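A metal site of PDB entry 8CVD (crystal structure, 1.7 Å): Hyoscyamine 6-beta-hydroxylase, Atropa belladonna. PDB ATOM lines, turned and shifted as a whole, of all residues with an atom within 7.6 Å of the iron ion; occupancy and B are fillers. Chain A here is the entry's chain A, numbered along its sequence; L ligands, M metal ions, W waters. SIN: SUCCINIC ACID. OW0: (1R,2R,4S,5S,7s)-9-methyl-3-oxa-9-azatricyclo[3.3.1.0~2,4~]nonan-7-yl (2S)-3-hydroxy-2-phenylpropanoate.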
ATOM      1  N   GLU A 116     -10.804 -13.032 -18.724  1.00  0.00           N
ATOM      2  CA  GLU A 116     -11.584 -13.669 -19.801  1.00  0.00           C
ATOM      3  C   GLU A 116     -12.815 -14.355 -19.202  1.00  0.00           C
ATOM      4  O   GLU A 116     -12.747 -14.794 -18.039  1.00  0.00           O
ATOM      5  CB  GLU A 116     -10.720 -14.668 -20.574  1.00  0.00           C
ATOM      6  CG  GLU A 116     -11.341 -15.107 -21.883  1.00  0.00           C
ATOM      7  CD  GLU A 116     -10.485 -16.044 -22.712  1.00  0.00           C
ATOM      8  OE1 GLU A 116      -9.405 -16.464 -22.232  1.00  0.00           O
ATOM      9  OE2 GLU A 116     -10.889 -16.340 -23.864  1.00  0.00           O
ATOM     10  N   LEU A 198       0.385 -16.573 -24.939  1.00  0.00           N
ATOM     11  CA  LEU A 198      -0.520 -16.497 -23.762  1.00  0.00           C
ATOM     12  C   LEU A 198       0.070 -17.384 -22.675  1.00  0.00           C
ATOM     13  O   LEU A 198       0.064 -18.614 -22.866  1.00  0.00           O
ATOM     14  CB  LEU A 198      -1.916 -16.945 -24.164  1.00  0.00           C
ATOM     15  CG  LEU A 198      -2.788 -15.852 -24.781  1.00  0.00           C
ATOM     16  CD1 LEU A 198      -2.178 -15.335 -26.066  1.00  0.00           C
ATOM     17  CD2 LEU A 198      -4.205 -16.364 -25.025  1.00  0.00           C
ATOM     18  N   ASN A 200      -0.787 -18.730 -19.231  1.00  0.00           N
ATOM     19  CA  ASN A 200      -2.060 -18.896 -18.487  1.00  0.00           C
ATOM     20  C   ASN A 200      -1.731 -19.388 -17.079  1.00  0.00           C
ATOM     21  O   ASN A 200      -1.033 -20.398 -16.958  1.00  0.00           O
ATOM     22  CB  ASN A 200      -2.995 -19.871 -19.198  1.00  0.00           C
ATOM     23  CG  ASN A 200      -3.187 -19.487 -20.644  1.00  0.00           C
ATOM     24  OD1 ASN A 200      -3.667 -18.387 -20.923  1.00  0.00           O
ATOM     25  ND2 ASN A 200      -2.811 -20.370 -21.558  1.00  0.00           N
ATOM     26  N   TYR A 202      -3.517 -20.659 -13.611  1.00  0.00           N
ATOM     27  CA  TYR A 202      -4.733 -21.221 -12.965  1.00  0.00           C
ATOM     28  C   TYR A 202      -4.411 -21.428 -11.491  1.00  0.00           C
ATOM     29  O   TYR A 202      -3.793 -22.429 -11.133  1.00  0.00           O
ATOM     30  CB  TYR A 202      -5.135 -22.517 -13.654  1.00  0.00           C
ATOM     31  CG  TYR A 202      -5.255 -22.406 -15.150  1.00  0.00           C
ATOM     32  CD1 TYR A 202      -6.433 -21.981 -15.746  1.00  0.00           C
ATOM     33  CD2 TYR A 202      -4.173 -22.711 -15.968  1.00  0.00           C
ATOM     34  CE1 TYR A 202      -6.533 -21.868 -17.120  1.00  0.00           C
ATOM     35  CE2 TYR A 202      -4.266 -22.603 -17.347  1.00  0.00           C
ATOM     36  CZ  TYR A 202      -5.454 -22.189 -17.926  1.00  0.00           C
ATOM     37  OH  TYR A 202      -5.550 -22.088 -19.282  1.00  0.00           O
ATOM     38  N   SER A 214     -10.977 -22.416 -18.461  1.00  0.00           N
ATOM     39  CA  SER A 214     -11.506 -21.846 -19.724  1.00  0.00           C
ATOM     40  C   SER A 214     -12.652 -22.736 -20.215  1.00  0.00           C
ATOM     41  O   SER A 214     -12.552 -23.967 -20.087  1.00  0.00           O
ATOM     42  CB  SER A 214     -10.435 -21.694 -20.781  1.00  0.00           C
ATOM     43  OG  SER A 214      -9.874 -22.947 -21.120  1.00  0.00           O
ATOM     44  N   GLY A 215     -13.707 -22.120 -20.749  1.00  0.00           N
ATOM     45  CA  GLY A 215     -14.830 -22.828 -21.382  1.00  0.00           C
ATOM     46  C   GLY A 215     -14.353 -23.522 -22.636  1.00  0.00           C
ATOM     47  O   GLY A 215     -13.258 -23.180 -23.133  1.00  0.00           O
ATOM     48  N   HIS A 217     -13.803 -24.303 -26.377  1.00  0.00           N
ATOM     49  CA  HIS A 217     -13.580 -23.381 -27.523  1.00  0.00           C
ATOM     50  C   HIS A 217     -12.647 -24.020 -28.542  1.00  0.00           C
ATOM     51  O   HIS A 217     -11.756 -24.795 -28.138  1.00  0.00           O
ATOM     52  CB  HIS A 217     -13.030 -22.040 -27.019  1.00  0.00           C
ATOM     53  CG  HIS A 217     -11.651 -22.128 -26.450  1.00  0.00           C
ATOM     54  ND1 HIS A 217     -11.410 -22.605 -25.176  1.00  0.00           N
ATOM     55  CD2 HIS A 217     -10.438 -21.824 -26.967  1.00  0.00           C
ATOM     56  CE1 HIS A 217     -10.114 -22.591 -24.943  1.00  0.00           C
ATOM     57  NE2 HIS A 217      -9.494 -22.109 -26.023  1.00  0.00           N
ATOM     58  N   TYR A 218     -12.811 -23.658 -29.811  1.00  0.00           N
ATOM     59  CA  TYR A 218     -11.701 -23.652 -30.800  1.00  0.00           C
ATOM     60  C   TYR A 218     -10.818 -22.448 -30.499  1.00  0.00           C
ATOM     61  O   TYR A 218     -11.349 -21.380 -30.143  1.00  0.00           O
ATOM     62  CB  TYR A 218     -12.199 -23.450 -32.228  1.00  0.00           C
ATOM     63  CG  TYR A 218     -13.070 -24.519 -32.813  1.00  0.00           C
ATOM     64  CD1 TYR A 218     -12.524 -25.699 -33.308  1.00  0.00           C
ATOM     65  CD2 TYR A 218     -14.430 -24.330 -32.951  1.00  0.00           C
ATOM     66  CE1 TYR A 218     -13.323 -26.663 -33.888  1.00  0.00           C
ATOM     67  CE2 TYR A 218     -15.243 -25.292 -33.533  1.00  0.00           C
ATOM     68  CZ  TYR A 218     -14.682 -26.465 -34.015  1.00  0.00           C
ATOM     69  OH  TYR A 218     -15.472 -27.418 -34.596  1.00  0.00           O
ATOM     70  N   ASP A 219      -9.501 -22.586 -30.668  1.00  0.00           N
ATOM     71  CA  ASP A 219      -8.629 -21.402 -30.870  1.00  0.00           C
ATOM     72  C   ASP A 219      -9.034 -20.822 -32.236  1.00  0.00           C
ATOM     73  O   ASP A 219      -9.170 -21.599 -33.195  1.00  0.00           O
ATOM     74  CB  ASP A 219      -7.155 -21.763 -30.774  1.00  0.00           C
ATOM     75  CG  ASP A 219      -6.667 -21.993 -29.352  1.00  0.00           C
ATOM     76  OD1 ASP A 219      -7.487 -21.850 -28.427  1.00  0.00           O
ATOM     77  OD2 ASP A 219      -5.488 -22.329 -29.200  1.00  0.00           O
ATOM     78  N   GLY A 220      -9.270 -19.510 -32.313  1.00  0.00           N
ATOM     79  CA  GLY A 220      -9.807 -18.880 -33.534  1.00  0.00           C
ATOM     80  C   GLY A 220      -8.770 -18.737 -34.627  1.00  0.00           C
ATOM     81  O   GLY A 220      -9.158 -18.585 -35.796  1.00  0.00           O
ATOM     82  N   ASN A 221      -7.486 -18.840 -34.267  1.00  0.00           N
ATOM     83  CA  ASN A 221      -6.312 -18.587 -35.137  1.00  0.00           C
ATOM     84  C   ASN A 221      -6.026 -19.823 -36.016  1.00  0.00           C
ATOM     85  O   ASN A 221      -6.918 -20.668 -36.157  1.00  0.00           O
ATOM     86  CB  ASN A 221      -5.124 -18.163 -34.278  1.00  0.00           C
ATOM     87  CG  ASN A 221      -4.892 -19.102 -33.119  1.00  0.00           C
ATOM     88  OD1 ASN A 221      -5.710 -19.149 -32.190  1.00  0.00           O
ATOM     89  ND2 ASN A 221      -3.817 -19.869 -33.166  1.00  0.00           N
ATOM     90  N   THR A 224      -2.067 -23.556 -32.809  1.00  0.00           N
ATOM     91  CA  THR A 224      -1.552 -23.231 -31.461  1.00  0.00           C
ATOM     92  C   THR A 224      -0.637 -24.358 -30.990  1.00  0.00           C
ATOM     93  O   THR A 224      -1.031 -25.524 -31.134  1.00  0.00           O
ATOM     94  CB  THR A 224      -2.699 -23.000 -30.475  1.00  0.00           C
ATOM     95  OG1 THR A 224      -3.513 -21.935 -30.965  1.00  0.00           O
ATOM     96  CG2 THR A 224      -2.212 -22.699 -29.080  1.00  0.00           C
ATOM     97  N   LEU A 226       1.045 -25.618 -27.427  1.00  0.00           N
ATOM     98  CA  LEU A 226       0.751 -25.448 -25.989  1.00  0.00           C
ATOM     99  C   LEU A 226       1.746 -26.304 -25.203  1.00  0.00           C
ATOM    100  O   LEU A 226       1.906 -27.494 -25.530  1.00  0.00           O
ATOM    101  CB  LEU A 226      -0.707 -25.864 -25.760  1.00  0.00           C
ATOM    102  CG  LEU A 226      -1.163 -25.916 -24.304  1.00  0.00           C
ATOM    103  CD1 LEU A 226      -1.078 -24.551 -23.657  1.00  0.00           C
ATOM    104  CD2 LEU A 226      -2.580 -26.465 -24.233  1.00  0.00           C
ATOM    105  N   LEU A 233      -6.038 -29.801 -19.068  1.00  0.00           N
ATOM    106  CA  LEU A 233      -6.499 -29.627 -20.474  1.00  0.00           C
ATOM    107  C   LEU A 233      -7.396 -30.812 -20.835  1.00  0.00           C
ATOM    108  O   LEU A 233      -6.994 -31.976 -20.592  1.00  0.00           O
ATOM    109  CB  LEU A 233      -5.296 -29.551 -21.414  1.00  0.00           C
ATOM    110  CG  LEU A 233      -5.635 -29.358 -22.895  1.00  0.00           C
ATOM    111  CD1 LEU A 233      -6.243 -27.986 -23.138  1.00  0.00           C
ATOM    112  CD2 LEU A 233      -4.397 -29.543 -23.750  1.00  0.00           C
ATOM    113  N   ASN A 255      -2.857 -27.714 -31.242  1.00  0.00           N
ATOM    114  CA  ASN A 255      -4.315 -27.455 -31.367  1.00  0.00           C
ATOM    115  C   ASN A 255      -4.560 -26.804 -32.731  1.00  0.00           C
ATOM    116  O   ASN A 255      -4.105 -25.677 -32.917  1.00  0.00           O
ATOM    117  CB  ASN A 255      -4.834 -26.567 -30.236  1.00  0.00           C
ATOM    118  CG  ASN A 255      -4.981 -27.269 -28.905  1.00  0.00           C
ATOM    119  OD1 ASN A 255      -5.511 -28.373 -28.824  1.00  0.00           O
ATOM    120  ND2 ASN A 255      -4.557 -26.629 -27.834  1.00  0.00           N
ATOM    121  N   SER A 271      -9.388 -28.290 -32.907  1.00  0.00           N
ATOM    122  CA  SER A 271      -9.378 -28.757 -31.498  1.00  0.00           C
ATOM    123  C   SER A 271     -10.380 -27.946 -30.672  1.00  0.00           C
ATOM    124  O   SER A 271     -10.150 -26.741 -30.470  1.00  0.00           O
ATOM    125  CB  SER A 271      -7.997 -28.666 -30.898  1.00  0.00           C
ATOM    126  OG  SER A 271      -8.062 -28.865 -29.495  1.00  0.00           O
ATOM    127  N   ILE A 272     -11.444 -28.574 -30.186  1.00  0.00           N
ATOM    128  CA  ILE A 272     -12.327 -27.975 -29.156  1.00  0.00           C
ATOM    129  C   ILE A 272     -11.797 -28.446 -27.800  1.00  0.00           C
ATOM    130  O   ILE A 272     -11.825 -29.658 -27.547  1.00  0.00           O
ATOM    131  CB  ILE A 272     -13.800 -28.363 -29.370  1.00  0.00           C
ATOM    132  CG1 ILE A 272     -14.316 -27.848 -30.716  1.00  0.00           C
ATOM    133  CG2 ILE A 272     -14.643 -27.867 -28.198  1.00  0.00           C
ATOM    134  CD1 ILE A 272     -15.672 -28.410 -31.121  1.00  0.00           C
ATOM    135  N   HIS A 273     -11.299 -27.514 -26.993  1.00  0.00           N
ATOM    136  CA  HIS A 273     -10.626 -27.818 -25.700  1.00  0.00           C
ATOM    137  C   HIS A 273     -11.143 -26.886 -24.612  1.00  0.00           C
ATOM    138  O   HIS A 273     -11.712 -25.825 -24.930  1.00  0.00           O
ATOM    139  CB  HIS A 273      -9.098 -27.781 -25.853  1.00  0.00           C
ATOM    140  CG  HIS A 273      -8.581 -26.497 -26.396  1.00  0.00           C
ATOM    141  ND1 HIS A 273      -8.457 -26.263 -27.756  1.00  0.00           N
ATOM    142  CD2 HIS A 273      -8.147 -25.370 -25.784  1.00  0.00           C
ATOM    143  CE1 HIS A 273      -8.002 -25.046 -27.958  1.00  0.00           C
ATOM    144  NE2 HIS A 273      -7.790 -24.473 -26.763  1.00  0.00           N
ATOM    145  N   ARG A 274     -10.932 -27.285 -23.361  1.00  0.00           N
ATOM    146  CA  ARG A 274     -11.272 -26.503 -22.155  1.00  0.00           C
ATOM    147  C   ARG A 274     -10.194 -26.803 -21.114  1.00  0.00           C
ATOM    148  O   ARG A 274      -9.431 -27.765 -21.293  1.00  0.00           O
ATOM    149  CB  ARG A 274     -12.675 -26.854 -21.665  1.00  0.00           C
ATOM    150  CG  ARG A 274     -12.769 -28.175 -20.913  1.00  0.00           C
ATOM    151  CD  ARG A 274     -14.194 -28.464 -20.497  1.00  0.00           C
ATOM    152  NE  ARG A 274     -14.292 -29.764 -19.851  1.00  0.00           N
ATOM    153  CZ  ARG A 274     -15.440 -30.362 -19.528  1.00  0.00           C
ATOM    154  NH1 ARG A 274     -16.597 -29.773 -19.778  1.00  0.00           N
ATOM    155  NH2 ARG A 274     -15.423 -31.545 -18.933  1.00  0.00           N
ATOM    156  N   VAL A 275     -10.146 -25.992 -20.052  1.00  0.00           N
ATOM    157  CA  VAL A 275      -9.255 -26.235 -18.887  1.00  0.00           C
ATOM    158  C   VAL A 275     -10.101 -26.259 -17.625  1.00  0.00           C
ATOM    159  O   VAL A 275     -10.912 -25.322 -17.425  1.00  0.00           O
ATOM    160  CB  VAL A 275      -8.143 -25.185 -18.807  1.00  0.00           C
ATOM    161  CG1 VAL A 275      -7.213 -25.458 -17.638  1.00  0.00           C
ATOM    162  CG2 VAL A 275      -7.376 -25.089 -20.112  1.00  0.00           C
ATOM    163  N   ALA A 287       0.803 -21.019 -24.217  1.00  0.00           N
ATOM    164  CA  ALA A 287       0.157 -21.186 -25.531  1.00  0.00           C
ATOM    165  C   ALA A 287       0.759 -20.185 -26.511  1.00  0.00           C
ATOM    166  O   ALA A 287       0.724 -18.976 -26.194  1.00  0.00           O
ATOM    167  CB  ALA A 287      -1.331 -21.011 -25.392  1.00  0.00           C
ATOM    168  N   LEU A 289      -0.118 -18.875 -30.019  1.00  0.00           N
ATOM    169  CA  LEU A 289      -1.243 -18.808 -30.976  1.00  0.00           C
ATOM    170  C   LEU A 289      -0.749 -18.083 -32.221  1.00  0.00           C
ATOM    171  O   LEU A 289      -0.507 -16.868 -32.153  1.00  0.00           O
ATOM    172  CB  LEU A 289      -2.445 -18.084 -30.344  1.00  0.00           C
ATOM    173  CG  LEU A 289      -3.238 -18.907 -29.332  1.00  0.00           C
ATOM    174  CD1 LEU A 289      -2.504 -19.025 -28.016  1.00  0.00           C
ATOM    175  CD2 LEU A 289      -4.610 -18.284 -29.117  1.00  0.00           C
ATOM    176  N   TYR A 325     -15.955 -14.019 -32.827  1.00  0.00           N
ATOM    177  CA  TYR A 325     -15.263 -15.122 -32.105  1.00  0.00           C
ATOM    178  C   TYR A 325     -15.057 -14.743 -30.634  1.00  0.00           C
ATOM    179  O   TYR A 325     -15.244 -15.603 -29.744  1.00  0.00           O
ATOM    180  CB  TYR A 325     -13.942 -15.445 -32.803  1.00  0.00           C
ATOM    181  CG  TYR A 325     -13.065 -16.362 -31.992  1.00  0.00           C
ATOM    182  CD1 TYR A 325     -13.405 -17.696 -31.828  1.00  0.00           C
ATOM    183  CD2 TYR A 325     -11.925 -15.891 -31.363  1.00  0.00           C
ATOM    184  CE1 TYR A 325     -12.623 -18.547 -31.056  1.00  0.00           C
ATOM    185  CE2 TYR A 325     -11.135 -16.730 -30.591  1.00  0.00           C
ATOM    186  CZ  TYR A 325     -11.480 -18.061 -30.440  1.00  0.00           C
ATOM    187  OH  TYR A 325     -10.692 -18.871 -29.681  1.00  0.00           O
HETATM  188  C1  SIN L   1      -4.252 -24.718 -21.384  1.00  0.00           C
HETATM  189  O1  SIN L   1      -3.805 -25.873 -21.348  1.00  0.00           O
HETATM  190  O2  SIN L   1      -4.062 -23.894 -20.482  1.00  0.00           O
HETATM  191  C2  SIN L   1      -5.110 -24.313 -22.579  1.00  0.00           C
HETATM  192  C3  SIN L   1      -4.884 -22.933 -23.157  1.00  0.00           C
HETATM  193  C4  SIN L   1      -5.798 -22.601 -24.328  1.00  0.00           C
HETATM  194  O3  SIN L   1      -7.024 -22.732 -24.169  1.00  0.00           O
HETATM  195  O4  SIN L   1      -5.280 -22.228 -25.409  1.00  0.00           O
HETATM  196  N1  OW0 L   2      -9.202 -18.068 -24.980  1.00  0.00           N
HETATM  197  C2  OW0 L   2      -8.355 -18.911 -27.002  1.00  0.00           C
HETATM  198  C4  OW0 L   2      -9.591 -18.331 -26.382  1.00  0.00           C
HETATM  199  C5  OW0 L   2      -7.955 -16.081 -25.704  1.00  0.00           C
HETATM  200  C6  OW0 L   2      -9.984 -17.012 -27.032  1.00  0.00           C
HETATM  201  C8  OW0 L   2      -9.318 -19.210 -24.071  1.00  0.00           C
HETATM  202  O2  OW0 L   2      -8.000 -16.174 -28.147  1.00  0.00           O
HETATM  203  O3  OW0 L   2      -4.713 -14.836 -31.244  1.00  0.00           O
HETATM  204  O4  OW0 L   2      -7.389 -14.026 -28.057  1.00  0.00           O
HETATM  205  C11 OW0 L   2      -7.519 -14.910 -31.119  1.00  0.00           C
HETATM  206  C12 OW0 L   2      -7.681 -15.738 -32.216  1.00  0.00           C
HETATM  207  C13 OW0 L   2      -8.447 -15.333 -33.306  1.00  0.00           C
HETATM  208  C14 OW0 L   2      -9.049 -14.092 -33.305  1.00  0.00           C
HETATM  209  C15 OW0 L   2      -8.884 -13.257 -32.232  1.00  0.00           C
HETATM  210  C9  OW0 L   2      -7.378 -15.080 -28.628  1.00  0.00           C
HETATM  211  C1  OW0 L   2      -7.232 -18.391 -26.233  1.00  0.00           C
HETATM  212  C3  OW0 L   2      -7.839 -17.505 -25.177  1.00  0.00           C
HETATM  213  C7  OW0 L   2      -8.838 -15.980 -26.966  1.00  0.00           C
HETATM  214  O1  OW0 L   2      -7.567 -19.792 -26.170  1.00  0.00           O
HETATM  215  C10 OW0 L   2      -6.664 -15.348 -29.935  1.00  0.00           C
HETATM  216  C16 OW0 L   2      -8.132 -13.651 -31.131  1.00  0.00           C
HETATM  217  C17 OW0 L   2      -5.289 -14.704 -29.944  1.00  0.00           C
HETATM  218 FE    FE M   1      -7.441 -22.424 -26.425  1.00  0.00          FE
HETATM  219  O   HOH W   1      -4.583 -24.004 -27.004  1.00  0.00           O
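Water W1 bridges the side-chain amide nitrogen (ND2) of Asn 255 (2.8 Å) and the side-chain carboxylate (OD2) of Asp 219 (2.9 Å).
Within 4 Å of the iron ion: His 217, Asp 219 and His 273. The nearest printed residue that does not touch the iron ion is Asn 255 (5.3 Å).
The iron ion is bound by the side-chain carboxylate (OD1) of Asp 219 (2.1 Å), a ring nitrogen (NE2) of His 273 (2.1 Å), a ring nitrogen (NE2) of His 217 (2.1 Å), an oxygen (O3) of SIN L1 (2.3 Å) and an oxygen (O4) of SIN L1 (2.4 Å). Slightly farther from the iron ion lies O1 of OW0 L2 (2.6 Å).
A nitrogen (N1) of OW0 L2 lies within salt-bridge range of the side-chain carboxylate (OE2) of Glu 116 (2.7 Å). A ring nitrogen (NE2) of His 217 lies close to an oxygen (O1) of OW0 L2 (3.0 Å).
OG1 of Thr 224 sits at hydrogen-bond distance from OD2 of Asp 219 (2.7 Å). A ring nitrogen (ND1) of His 273 sits at hydrogen-bond distance from the side-chain hydroxyl (OG) of Ser 271 (3.2 Å). The backbone carbonyl oxygen of Gly 215 sits at hydrogen-bond distance from a ring nitrogen (ND1) of His 217, 2.8 Å away.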
